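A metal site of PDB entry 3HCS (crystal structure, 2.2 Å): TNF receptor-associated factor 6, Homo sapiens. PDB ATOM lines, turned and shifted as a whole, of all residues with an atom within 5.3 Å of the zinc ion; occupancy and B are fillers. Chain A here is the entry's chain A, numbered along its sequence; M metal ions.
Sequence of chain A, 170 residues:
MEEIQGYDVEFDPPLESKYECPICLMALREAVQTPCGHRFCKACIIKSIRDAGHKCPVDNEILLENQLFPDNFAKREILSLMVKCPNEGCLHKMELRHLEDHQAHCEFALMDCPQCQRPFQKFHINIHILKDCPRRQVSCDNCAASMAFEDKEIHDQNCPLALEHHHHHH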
ATOM      1  N   CYS A 140     -28.702   9.893   9.045  1.00  0.00           N
ATOM      2  CA  CYS A 140     -27.716  10.733   9.720  1.00  0.00           C
ATOM      3  C   CYS A 140     -26.311  10.176   9.516  1.00  0.00           C
ATOM      4  O   CYS A 140     -26.091   8.979   9.703  1.00  0.00           O
ATOM      5  CB  CYS A 140     -28.029  10.802  11.217  1.00  0.00           C
ATOM      6  SG  CYS A 140     -26.748  11.598  12.186  1.00  0.00           S
ATOM      7  N   ASN A 142     -23.831  10.520  11.338  1.00  0.00           N
ATOM      8  CA  ASN A 142     -23.255  10.086  12.604  1.00  0.00           C
ATOM      9  C   ASN A 142     -23.843   8.856  13.266  1.00  0.00           C
ATOM     10  O   ASN A 142     -23.101   7.934  13.625  1.00  0.00           O
ATOM     11  CB  ASN A 142     -23.277  11.256  13.585  1.00  0.00           C
ATOM     12  CG  ASN A 142     -22.519  12.454  13.064  1.00  0.00           C
ATOM     13  OD1 ASN A 142     -21.340  12.353  12.730  1.00  0.00           O
ATOM     14  ND2 ASN A 142     -23.195  13.590  12.991  1.00  0.00           N
ATOM     15  N   CYS A 143     -25.161   8.813  13.440  1.00  0.00           N
ATOM     16  CA  CYS A 143     -25.775   7.666  14.107  1.00  0.00           C
ATOM     17  C   CYS A 143     -26.579   6.727  13.218  1.00  0.00           C
ATOM     18  O   CYS A 143     -27.199   5.785  13.705  1.00  0.00           O
ATOM     19  CB  CYS A 143     -26.662   8.135  15.264  1.00  0.00           C
ATOM     20  SG  CYS A 143     -28.286   8.753  14.778  1.00  0.00           S
ATOM     21  N   ALA A 144     -26.588   6.990  11.905  1.00  0.00           N
ATOM     22  CA  ALA A 144     -27.324   6.138  10.985  1.00  0.00           C
ATOM     23  C   ALA A 144     -28.837   6.124  11.255  1.00  0.00           C
ATOM     24  O   ALA A 144     -29.542   5.185  10.880  1.00  0.00           O
ATOM     25  CB  ALA A 144     -26.784   4.708  11.057  1.00  0.00           C
ATOM     26  N   ALA A 145     -29.316   7.145  11.951  1.00  0.00           N
ATOM     27  CA  ALA A 145     -30.753   7.241  12.213  1.00  0.00           C
ATOM     28  C   ALA A 145     -31.442   7.726  10.947  1.00  0.00           C
ATOM     29  O   ALA A 145     -30.902   8.560  10.222  1.00  0.00           O
ATOM     30  CB  ALA A 145     -31.023   8.207  13.355  1.00  0.00           C
ATOM     31  N   MET A 147     -34.633   9.659   9.206  1.00  0.00           N
ATOM     32  CA  MET A 147     -35.621  10.667   9.555  1.00  0.00           C
ATOM     33  C   MET A 147     -36.177  11.363   8.323  1.00  0.00           C
ATOM     34  O   MET A 147     -35.717  11.125   7.204  1.00  0.00           O
ATOM     35  CB  MET A 147     -34.990  11.703  10.481  1.00  0.00           C
ATOM     36  CG  MET A 147     -33.832  12.448   9.841  1.00  0.00           C
ATOM     37  SD  MET A 147     -32.692  13.076  11.058  1.00  0.00           S
ATOM     38  CE  MET A 147     -31.802  11.558  11.486  1.00  0.00           C
ATOM     39  N   HIS A 155     -32.475  17.411  14.201  1.00  0.00           N
ATOM     40  CA  HIS A 155     -31.783  16.195  14.612  1.00  0.00           C
ATOM     41  C   HIS A 155     -30.273  16.440  14.715  1.00  0.00           C
ATOM     42  O   HIS A 155     -29.612  16.057  15.686  1.00  0.00           O
ATOM     43  CB  HIS A 155     -32.008  15.071  13.605  1.00  0.00           C
ATOM     44  CG  HIS A 155     -31.172  13.870  13.882  1.00  0.00           C
ATOM     45  ND1 HIS A 155     -31.571  12.865  14.732  1.00  0.00           N
ATOM     46  CD2 HIS A 155     -29.918  13.547  13.477  1.00  0.00           C
ATOM     47  CE1 HIS A 155     -30.598  11.972  14.851  1.00  0.00           C
ATOM     48  NE2 HIS A 155     -29.585  12.374  14.105  1.00  0.00           N
ATOM     49  N   CYS A 159     -27.868  15.882  17.790  1.00  0.00           N
ATOM     50  CA  CYS A 159     -27.538  14.491  17.574  1.00  0.00           C
ATOM     51  C   CYS A 159     -26.458  14.032  18.535  1.00  0.00           C
ATOM     52  O   CYS A 159     -25.547  14.785  18.867  1.00  0.00           O
ATOM     53  CB  CYS A 159     -27.063  14.284  16.131  1.00  0.00           C
ATOM     54  SG  CYS A 159     -26.351  12.669  15.826  1.00  0.00           S
ATOM     55  N   PRO A 160     -26.540  12.778  19.019  1.00  0.00           N
ATOM     56  CA  PRO A 160     -25.536  12.260  19.944  1.00  0.00           C
ATOM     57  C   PRO A 160     -24.161  12.222  19.268  1.00  0.00           C
ATOM     58  O   PRO A 160     -23.177  11.793  19.865  1.00  0.00           O
ATOM     59  CB  PRO A 160     -26.054  10.863  20.271  1.00  0.00           C
ATOM     60  CG  PRO A 160     -27.536  11.005  20.116  1.00  0.00           C
ATOM     61  CD  PRO A 160     -27.647  11.825  18.856  1.00  0.00           C
HETATM   62 ZN    ZN M   1     -27.812  11.109  14.420  1.00  0.00          ZN
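SG of Cys 143 lies close to N of Ala 145, 3.4 Å away. N of Cys 140 sits at hydrogen-bond distance from O of Ala 145 (2.8 Å). The side-chain sulfur (SG) of Cys 140 sits close to the backbone NH (N) of Asn 142 (3.2 Å).
The nearest printed residue that does not touch the zinc ion is Ala 145 (4.5 Å).
NE2 of His 155 is bound to the zinc ion. The zinc ion is bound by SG of Cys 143, at 2.4 Å. SG of Cys 140 is bound to the zinc ion. The zinc ion is bound by SG of Cys 159 (2.6 Å).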
